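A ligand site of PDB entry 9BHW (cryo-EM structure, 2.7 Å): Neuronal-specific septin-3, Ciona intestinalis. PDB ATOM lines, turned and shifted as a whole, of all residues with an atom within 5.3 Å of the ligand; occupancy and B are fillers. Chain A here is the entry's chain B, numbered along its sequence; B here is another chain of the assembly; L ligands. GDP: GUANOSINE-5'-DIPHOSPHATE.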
ATOM      1  N   SER A  36      -5.490  21.170   2.190  1.00  0.00           N
ATOM      2  CA  SER A  36      -6.762  21.711   2.617  1.00  0.00           C
ATOM      3  C   SER A  36      -6.843  21.784   4.134  1.00  0.00           C
ATOM      4  O   SER A  36      -6.189  21.029   4.851  1.00  0.00           O
ATOM      5  CB  SER A  36      -7.915  20.878   2.075  1.00  0.00           C
ATOM      6  OG  SER A  36      -7.895  20.833   0.661  1.00  0.00           O
ATOM      7  N   ALA A  37      -7.655  22.719   4.625  1.00  0.00           N
ATOM      8  CA  ALA A  37      -7.818  22.891   6.055  1.00  0.00           C
ATOM      9  C   ALA A  37      -8.502  21.681   6.669  1.00  0.00           C
ATOM     10  O   ALA A  37      -9.482  21.165   6.132  1.00  0.00           O
ATOM     11  CB  ALA A  37      -8.616  24.150   6.345  1.00  0.00           C
ATOM     12  N   GLY A  38      -7.995  21.233   7.809  1.00  0.00           N
ATOM     13  CA  GLY A  38      -8.555  20.094   8.489  1.00  0.00           C
ATOM     14  C   GLY A  38      -7.952  18.761   8.115  1.00  0.00           C
ATOM     15  O   GLY A  38      -8.652  17.740   8.215  1.00  0.00           O
ATOM     16  N   LEU A  39      -6.695  18.725   7.674  1.00  0.00           N
ATOM     17  CA  LEU A  39      -6.042  17.484   7.291  1.00  0.00           C
ATOM     18  C   LEU A  39      -4.936  17.091   8.258  1.00  0.00           C
ATOM     19  O   LEU A  39      -4.295  16.048   8.062  1.00  0.00           O
ATOM     20  CB  LEU A  39      -5.483  17.594   5.879  1.00  0.00           C
ATOM     21  CG  LEU A  39      -6.477  17.493   4.731  1.00  0.00           C
ATOM     22  CD1 LEU A  39      -5.774  17.628   3.411  1.00  0.00           C
ATOM     23  CD2 LEU A  39      -7.233  16.188   4.808  1.00  0.00           C
ATOM     24  N   GLY A  40      -4.694  17.877   9.298  1.00  0.00           N
ATOM     25  CA  GLY A  40      -3.661  17.532  10.267  1.00  0.00           C
ATOM     26  C   GLY A  40      -2.305  18.142  10.008  1.00  0.00           C
ATOM     27  O   GLY A  40      -1.297  17.550  10.408  1.00  0.00           O
ATOM     28  N   LYS A  41      -2.244  19.298   9.346  1.00  0.00           N
ATOM     29  CA  LYS A  41      -0.958  19.911   9.048  1.00  0.00           C
ATOM     30  C   LYS A  41      -0.294  20.438  10.314  1.00  0.00           C
ATOM     31  O   LYS A  41       0.883  20.154  10.577  1.00  0.00           O
ATOM     32  CB  LYS A  41      -1.141  21.024   8.029  1.00  0.00           C
ATOM     33  CG  LYS A  41      -2.026  20.633   6.852  1.00  0.00           C
ATOM     34  CD  LYS A  41      -1.996  21.682   5.769  1.00  0.00           C
ATOM     35  CE  LYS A  41      -2.415  23.044   6.285  1.00  0.00           C
ATOM     36  NZ  LYS A  41      -3.888  23.175   6.391  1.00  0.00           N
ATOM     37  N   SER A  42      -1.034  21.193  11.131  1.00  0.00           N
ATOM     38  CA  SER A  42      -0.481  21.715  12.370  1.00  0.00           C
ATOM     39  C   SER A  42      -0.106  20.584  13.328  1.00  0.00           C
ATOM     40  O   SER A  42       0.965  20.611  13.945  1.00  0.00           O
ATOM     41  CB  SER A  42      -1.477  22.669  13.029  1.00  0.00           C
ATOM     42  OG  SER A  42      -1.850  23.695  12.140  1.00  0.00           O
ATOM     43  N   THR A  43      -0.978  19.590  13.453  1.00  0.00           N
ATOM     44  CA  THR A  43      -0.691  18.455  14.316  1.00  0.00           C
ATOM     45  C   THR A  43       0.533  17.689  13.835  1.00  0.00           C
ATOM     46  O   THR A  43       1.339  17.237  14.642  1.00  0.00           O
ATOM     47  CB  THR A  43      -1.909  17.539  14.406  1.00  0.00           C
ATOM     48  OG1 THR A  43      -3.077  18.324  14.655  1.00  0.00           O
ATOM     49  CG2 THR A  43      -1.738  16.553  15.524  1.00  0.00           C
ATOM     50  N   LEU A  44       0.697  17.539  12.518  1.00  0.00           N
ATOM     51  CA  LEU A  44       1.860  16.816  12.017  1.00  0.00           C
ATOM     52  C   LEU A  44       3.139  17.598  12.228  1.00  0.00           C
ATOM     53  O   LEU A  44       4.188  17.018  12.537  1.00  0.00           O
ATOM     54  CB  LEU A  44       1.688  16.454  10.547  1.00  0.00           C
ATOM     55  CG  LEU A  44       2.782  15.492  10.092  1.00  0.00           C
ATOM     56  CD1 LEU A  44       2.398  14.057  10.406  1.00  0.00           C
ATOM     57  CD2 LEU A  44       3.093  15.658   8.623  1.00  0.00           C
ATOM     58  N   ARG A  56      -1.003  27.969  14.551  1.00  0.00           N
ATOM     59  CA  ARG A  56      -2.292  27.801  15.207  1.00  0.00           C
ATOM     60  C   ARG A  56      -2.323  26.425  15.861  1.00  0.00           C
ATOM     61  O   ARG A  56      -2.092  25.409  15.183  1.00  0.00           O
ATOM     62  CB  ARG A  56      -3.431  27.944  14.202  1.00  0.00           C
ATOM     63  CG  ARG A  56      -4.819  27.814  14.787  1.00  0.00           C
ATOM     64  CD  ARG A  56      -5.831  27.560  13.710  1.00  0.00           C
ATOM     65  NE  ARG A  56      -5.503  26.364  12.940  1.00  0.00           N
ATOM     66  CZ  ARG A  56      -5.864  25.131  13.280  1.00  0.00           C
ATOM     67  NH1 ARG A  56      -6.576  24.892  14.365  1.00  0.00           N
ATOM     68  NH2 ARG A  56      -5.497  24.118  12.502  1.00  0.00           N
ATOM     69  N   PRO A  58      -4.008  23.085  17.344  1.00  0.00           N
ATOM     70  CA  PRO A  58      -5.205  22.384  16.870  1.00  0.00           C
ATOM     71  C   PRO A  58      -6.455  22.685  17.673  1.00  0.00           C
ATOM     72  O   PRO A  58      -7.562  22.489  17.155  1.00  0.00           O
ATOM     73  CB  PRO A  58      -4.821  20.901  16.976  1.00  0.00           C
ATOM     74  CG  PRO A  58      -3.346  20.874  16.999  1.00  0.00           C
ATOM     75  CD  PRO A  58      -2.830  22.206  17.427  1.00  0.00           C
ATOM     76  N   LYS A 173      -4.296  11.772   7.627  1.00  0.00           N
ATOM     77  CA  LYS A 173      -5.260  10.988   8.389  1.00  0.00           C
ATOM     78  C   LYS A 173      -5.360   9.562   7.852  1.00  0.00           C
ATOM     79  O   LYS A 173      -6.413   9.075   7.459  1.00  0.00           O
ATOM     80  CB  LYS A 173      -6.630  11.660   8.400  1.00  0.00           C
ATOM     81  CG  LYS A 173      -6.622  13.085   8.912  1.00  0.00           C
ATOM     82  CD  LYS A 173      -8.009  13.662   8.856  1.00  0.00           C
ATOM     83  CE  LYS A 173      -8.102  14.956   9.618  1.00  0.00           C
ATOM     84  NZ  LYS A 173      -9.490  15.485   9.615  1.00  0.00           N
ATOM     85  N   SER A 174      -4.213   8.875   7.852  1.00  0.00           N
ATOM     86  CA  SER A 174      -4.144   7.519   7.333  1.00  0.00           C
ATOM     87  C   SER A 174      -4.834   6.509   8.227  1.00  0.00           C
ATOM     88  O   SER A 174      -4.971   5.353   7.836  1.00  0.00           O
ATOM     89  CB  SER A 174      -2.693   7.100   7.128  1.00  0.00           C
ATOM     90  OG  SER A 174      -2.605   5.687   7.010  1.00  0.00           O
ATOM     91  N   ASP A 175      -5.278   6.961   9.386  1.00  0.00           N
ATOM     92  CA  ASP A 175      -5.947   6.108  10.386  1.00  0.00           C
ATOM     93  C   ASP A 175      -7.300   5.650   9.842  1.00  0.00           C
ATOM     94  O   ASP A 175      -7.777   4.671  10.340  1.00  0.00           O
ATOM     95  CB  ASP A 175      -5.972   6.802  11.750  1.00  0.00           C
ATOM     96  CG  ASP A 175      -6.435   8.232  11.892  1.00  0.00           C
ATOM     97  OD1 ASP A 175      -7.189   8.503  12.812  1.00  0.00           O
ATOM     98  OD2 ASP A 175      -5.937   9.070  11.161  1.00  0.00           O
ATOM     99  N   ILE A 229       0.464   8.690   7.030  1.00  0.00           N
ATOM    100  CA  ILE A 229       0.916   9.340   8.251  1.00  0.00           C
ATOM    101  C   ILE A 229      -0.249   9.518   9.213  1.00  0.00           C
ATOM    102  O   ILE A 229      -1.413   9.637   8.803  1.00  0.00           O
ATOM    103  CB  ILE A 229       1.572  10.709   7.953  1.00  0.00           C
ATOM    104  CG1 ILE A 229       0.543  11.644   7.321  1.00  0.00           C
ATOM    105  CG2 ILE A 229       2.773  10.543   7.062  1.00  0.00           C
ATOM    106  CD1 ILE A 229       0.935  13.088   7.332  1.00  0.00           C
ATOM    107  N   VAL A 230       0.083   9.527  10.498  1.00  0.00           N
ATOM    108  CA  VAL A 230      -0.840   9.885  11.575  1.00  0.00           C
ATOM    109  C   VAL A 230      -0.095  10.818  12.525  1.00  0.00           C
ATOM    110  O   VAL A 230       0.987  10.467  13.000  1.00  0.00           O
ATOM    111  CB  VAL A 230      -1.382   8.659  12.324  1.00  0.00           C
ATOM    112  CG1 VAL A 230      -2.222   9.087  13.501  1.00  0.00           C
ATOM    113  CG2 VAL A 230      -2.167   7.763  11.399  1.00  0.00           C
ATOM    114  N   GLY A 231      -0.673  11.974  12.796  1.00  0.00           N
ATOM    115  CA  GLY A 231      -0.083  12.962  13.685  1.00  0.00           C
ATOM    116  C   GLY A 231      -0.938  13.136  14.925  1.00  0.00           C
ATOM    117  O   GLY A 231      -2.164  13.159  14.843  1.00  0.00           O
ATOM    118  N   SER A 232      -0.272  13.277  16.069  1.00  0.00           N
ATOM    119  CA  SER A 232      -0.961  13.441  17.339  1.00  0.00           C
ATOM    120  C   SER A 232       0.039  13.879  18.391  1.00  0.00           C
ATOM    121  O   SER A 232       1.165  13.370  18.416  1.00  0.00           O
ATOM    122  CB  SER A 232      -1.637  12.134  17.774  1.00  0.00           C
ATOM    123  OG  SER A 232      -2.038  12.189  19.142  1.00  0.00           O
ATOM    124  N   ARG A 246      -3.642   8.033  18.772  1.00  0.00           N
ATOM    125  CA  ARG A 246      -5.025   8.504  18.744  1.00  0.00           C
ATOM    126  C   ARG A 246      -5.919   7.443  19.361  1.00  0.00           C
ATOM    127  O   ARG A 246      -5.755   6.261  19.057  1.00  0.00           O
ATOM    128  CB  ARG A 246      -5.466   8.803  17.317  1.00  0.00           C
ATOM    129  CG  ARG A 246      -4.759   9.965  16.671  1.00  0.00           C
ATOM    130  CD  ARG A 246      -5.373  10.288  15.334  1.00  0.00           C
ATOM    131  NE  ARG A 246      -6.797  10.561  15.435  1.00  0.00           N
ATOM    132  CZ  ARG A 246      -7.315  11.704  15.844  1.00  0.00           C
ATOM    133  NH1 ARG A 246      -6.545  12.701  16.246  1.00  0.00           N
ATOM    134  NH2 ARG A 246      -8.636  11.858  15.865  1.00  0.00           N
ATOM    135  N   THR B 156     -13.428  17.134   8.968  1.00  0.00           N
ATOM    136  CA  THR B 156     -12.271  18.018   9.046  1.00  0.00           C
ATOM    137  C   THR B 156     -11.974  18.464  10.476  1.00  0.00           C
ATOM    138  O   THR B 156     -10.808  18.470  10.886  1.00  0.00           O
ATOM    139  CB  THR B 156     -12.475  19.244   8.155  1.00  0.00           C
ATOM    140  OG1 THR B 156     -13.765  19.798   8.410  1.00  0.00           O
ATOM    141  CG2 THR B 156     -12.384  18.857   6.699  1.00  0.00           C
ATOM    142  N   GLY B 157     -12.994  18.844  11.229  1.00  0.00           N
ATOM    143  CA  GLY B 157     -12.824  19.228  12.613  1.00  0.00           C
ATOM    144  C   GLY B 157     -12.782  20.718  12.881  1.00  0.00           C
ATOM    145  O   GLY B 157     -12.450  21.108  14.003  1.00  0.00           O
ATOM    146  N   HIS B 158     -13.095  21.548  11.893  1.00  0.00           N
ATOM    147  CA  HIS B 158     -13.027  22.992  12.052  1.00  0.00           C
ATOM    148  C   HIS B 158     -14.374  23.675  11.907  1.00  0.00           C
ATOM    149  O   HIS B 158     -14.677  24.593  12.672  1.00  0.00           O
ATOM    150  CB  HIS B 158     -12.053  23.595  11.038  1.00  0.00           C
ATOM    151  CG  HIS B 158     -10.619  23.307  11.335  1.00  0.00           C
ATOM    152  ND1 HIS B 158     -10.017  23.669  12.521  1.00  0.00           N
ATOM    153  CD2 HIS B 158      -9.660  22.696  10.606  1.00  0.00           C
ATOM    154  CE1 HIS B 158      -8.756  23.291  12.503  1.00  0.00           C
ATOM    155  NE2 HIS B 158      -8.515  22.697  11.349  1.00  0.00           N
ATOM    156  N   THR B 186     -13.010   8.312  11.607  1.00  0.00           N
ATOM    157  CA  THR B 186     -11.734   8.997  11.666  1.00  0.00           C
ATOM    158  C   THR B 186     -11.686  10.130  12.692  1.00  0.00           C
ATOM    159  O   THR B 186     -10.752  10.933  12.658  1.00  0.00           O
ATOM    160  CB  THR B 186     -11.360   9.539  10.287  1.00  0.00           C
ATOM    161  OG1 THR B 186     -10.022  10.055  10.323  1.00  0.00           O
ATOM    162  CG2 THR B 186     -12.284  10.653   9.898  1.00  0.00           C
ATOM    163  N   MET B 187     -12.661  10.210  13.591  1.00  0.00           N
ATOM    164  CA  MET B 187     -12.645  11.213  14.643  1.00  0.00           C
ATOM    165  C   MET B 187     -12.787  10.557  16.005  1.00  0.00           C
ATOM    166  O   MET B 187     -13.520   9.583  16.164  1.00  0.00           O
ATOM    167  CB  MET B 187     -13.745  12.250  14.485  1.00  0.00           C
ATOM    168  CG  MET B 187     -13.623  13.138  13.287  1.00  0.00           C
ATOM    169  SD  MET B 187     -14.961  14.334  13.292  1.00  0.00           S
ATOM    170  CE  MET B 187     -16.322  13.283  12.823  1.00  0.00           C
ATOM    171  N   GLU B 191     -13.479  15.200  19.393  1.00  0.00           N
ATOM    172  CA  GLU B 191     -13.467  15.912  18.128  1.00  0.00           C
ATOM    173  C   GLU B 191     -14.839  15.902  17.481  1.00  0.00           C
ATOM    174  O   GLU B 191     -15.269  16.906  16.903  1.00  0.00           O
ATOM    175  CB  GLU B 191     -12.445  15.287  17.176  1.00  0.00           C
ATOM    176  CG  GLU B 191     -11.007  15.402  17.622  1.00  0.00           C
ATOM    177  CD  GLU B 191     -10.093  14.465  16.859  1.00  0.00           C
ATOM    178  OE1 GLU B 191     -10.595  13.759  15.958  1.00  0.00           O
ATOM    179  OE2 GLU B 191      -8.883  14.431  17.160  1.00  0.00           O
ATOM    180  N   ARG B 194     -17.007  18.478  19.301  1.00  0.00           N
ATOM    181  CA  ARG B 194     -16.606  19.845  18.976  1.00  0.00           C
ATOM    182  C   ARG B 194     -17.024  20.223  17.560  1.00  0.00           C
ATOM    183  O   ARG B 194     -17.511  21.331  17.321  1.00  0.00           O
ATOM    184  CB  ARG B 194     -15.097  20.002  19.154  1.00  0.00           C
ATOM    185  CG  ARG B 194     -14.598  21.414  18.960  1.00  0.00           C
ATOM    186  CD  ARG B 194     -13.212  21.592  19.548  1.00  0.00           C
ATOM    187  NE  ARG B 194     -12.186  20.975  18.724  1.00  0.00           N
ATOM    188  CZ  ARG B 194     -11.518  19.872  19.057  1.00  0.00           C
ATOM    189  NH1 ARG B 194     -11.751  19.246  20.207  1.00  0.00           N
ATOM    190  NH2 ARG B 194     -10.596  19.392  18.234  1.00  0.00           N
HETATM  191  PB  GDP L   1      -5.014  21.692   9.948  1.00  0.00           P
HETATM  192  O1B GDP L   1      -3.726  22.019  10.602  1.00  0.00           O
HETATM  193  O2B GDP L   1      -4.921  21.016   8.614  1.00  0.00           O
HETATM  194  O3B GDP L   1      -5.970  22.839   9.953  1.00  0.00           O
HETATM  195  O3A GDP L   1      -5.647  20.572  10.857  1.00  0.00           O
HETATM  196  PA  GDP L   1      -5.408  20.372  12.404  1.00  0.00           P
HETATM  197  O1A GDP L   1      -4.005  19.919  12.631  1.00  0.00           O
HETATM  198  O2A GDP L   1      -5.958  21.504  13.195  1.00  0.00           O
HETATM  199  O5' GDP L   1      -6.347  19.123  12.639  1.00  0.00           O
HETATM  200  C5' GDP L   1      -7.755  19.260  12.606  1.00  0.00           C
HETATM  201  C4' GDP L   1      -8.382  18.166  13.444  1.00  0.00           C
HETATM  202  O4' GDP L   1      -7.939  16.914  12.966  1.00  0.00           O
HETATM  203  C3' GDP L   1      -7.928  18.249  14.879  1.00  0.00           C
HETATM  204  O3' GDP L   1      -9.070  18.214  15.733  1.00  0.00           O
HETATM  205  C2' GDP L   1      -7.057  17.039  15.100  1.00  0.00           C
HETATM  206  O2' GDP L   1      -7.309  16.513  16.407  1.00  0.00           O
HETATM  207  C1' GDP L   1      -7.485  16.091  14.018  1.00  0.00           C
HETATM  208  N9  GDP L   1      -6.317  15.336  13.569  1.00  0.00           N
HETATM  209  C8  GDP L   1      -5.066  15.792  13.555  1.00  0.00           C
HETATM  210  N7  GDP L   1      -4.215  14.860  13.086  1.00  0.00           N
HETATM  211  C5  GDP L   1      -4.927  13.775  12.798  1.00  0.00           C
HETATM  212  C6  GDP L   1      -4.659  12.442  12.267  1.00  0.00           C
HETATM  213  O6  GDP L   1      -3.503  12.116  11.978  1.00  0.00           O
HETATM  214  N1  GDP L   1      -5.669  11.602  12.108  1.00  0.00           N
HETATM  215  C2  GDP L   1      -6.904  11.961  12.412  1.00  0.00           C
HETATM  216  N2  GDP L   1      -7.904  11.077  12.227  1.00  0.00           N
HETATM  217  N3  GDP L   1      -7.225  13.169  12.898  1.00  0.00           N
HETATM  218  C4  GDP L   1      -6.300  14.103  13.112  1.00  0.00           C
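NH2 of Arg 194 of chain B is in hydrogen-bond range of O3' of the ligand.
The backbone NH (N) of Gly 231 lies within hydrogen-bond range of an oxygen (O6) of the ligand (2.9 Å).
An oxygen (O2B) of the ligand sits at hydrogen-bond distance from the backbone NH (N) of Gly 38 (3.2 Å).
The backbone NH (N) of Ser 42 lies within hydrogen-bond range of an oxygen (O1B) of the ligand (2.9 Å).
N1 of the ligand is in hydrogen-bond range of OD2 of Asp 175 (2.7 Å).
A nitrogen (N2) of the ligand is in hydrogen-bond range of the side-chain hydroxyl (OG1) of Thr 186 of chain B, at 3.0 Å.
An oxygen (O2B) of the ligand lies within hydrogen-bond range of the backbone NH (N) of Gly 40.
An oxygen (O1B) of the ligand is in hydrogen-bond range of the side-chain hydroxyl of Ser 42.
OE2 of Glu 191 of chain B sits at hydrogen-bond distance from O2' of the ligand, 2.7 Å away.
O2A of the ligand is in salt-bridge range of NH2 of Arg 56 (2.7 Å).
An oxygen (O2B) of the ligand sits at hydrogen-bond distance from the backbone NH (N) of Lys 41 (3.3 Å).
The backbone NH (N) of Leu 39 lies within hydrogen-bond range of an oxygen (O2B) of the ligand (3.0 Å).
The backbone NH (N) of Thr 43 is in hydrogen-bond range of an oxygen (O1A) of the ligand, at 3.2 Å.
A nitrogen (N3) of the ligand sits close to the guanidinium group (NH1) of Arg 246 (3.4 Å).
An oxygen (O2B) of the ligand lies within salt-bridge range of the side-chain amino group of Lys 41, 3.3 Å away.
The side-chain hydroxyl (OG1) of Thr 43 is in hydrogen-bond range of an oxygen (O1A) of the ligand, at 2.7 Å.
O of Thr 186 of chain B sits at hydrogen-bond distance from N2 of the ligand.
An oxygen (O3B) of the ligand lies within hydrogen-bond range of a ring nitrogen (NE2) of His 158 of chain B, at 2.9 Å.
The side-chain carboxylate (OD1) of Asp 175 is in salt-bridge range of the guanidinium group (NE) of Arg 246, 3.4 Å away.
The backbone carbonyl oxygen (O) of Gly 38 is in hydrogen-bond range of the side-chain amino group (NZ) of Lys 173, 2.8 Å away.
The side-chain carboxylate of Glu 191 of chain B is in salt-bridge range of the guanidinium group of Arg 246, at 2.7 Å.
Merely in contact with the ligand: Val 230 (3.5 Å), Thr 156 of chain B (3.5 Å), Lys 173 (3.6 Å), Pro 58 (3.9 Å) and Ser 36 (3.97 Å).
Hydrophobic or aromatic side chains within 4 Å of the ligand: Pro 58, Val 230 and His 158 of chain B.
Within 4 Å of the ligand: Ser 36, Gly 38, Leu 39, Gly 40, Lys 41, Ser 42, Thr 43, Arg 56, Pro 58, Lys 173, Asp 175, Val 230, Gly 231, Arg 246, Thr 156 of chain B, His 158 of chain B, Thr 186 of chain B, Glu 191 of chain B and Arg 194 of chain B.
The nearest printed residue that does not touch the ligand is Ala 37 (4.1 Å).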
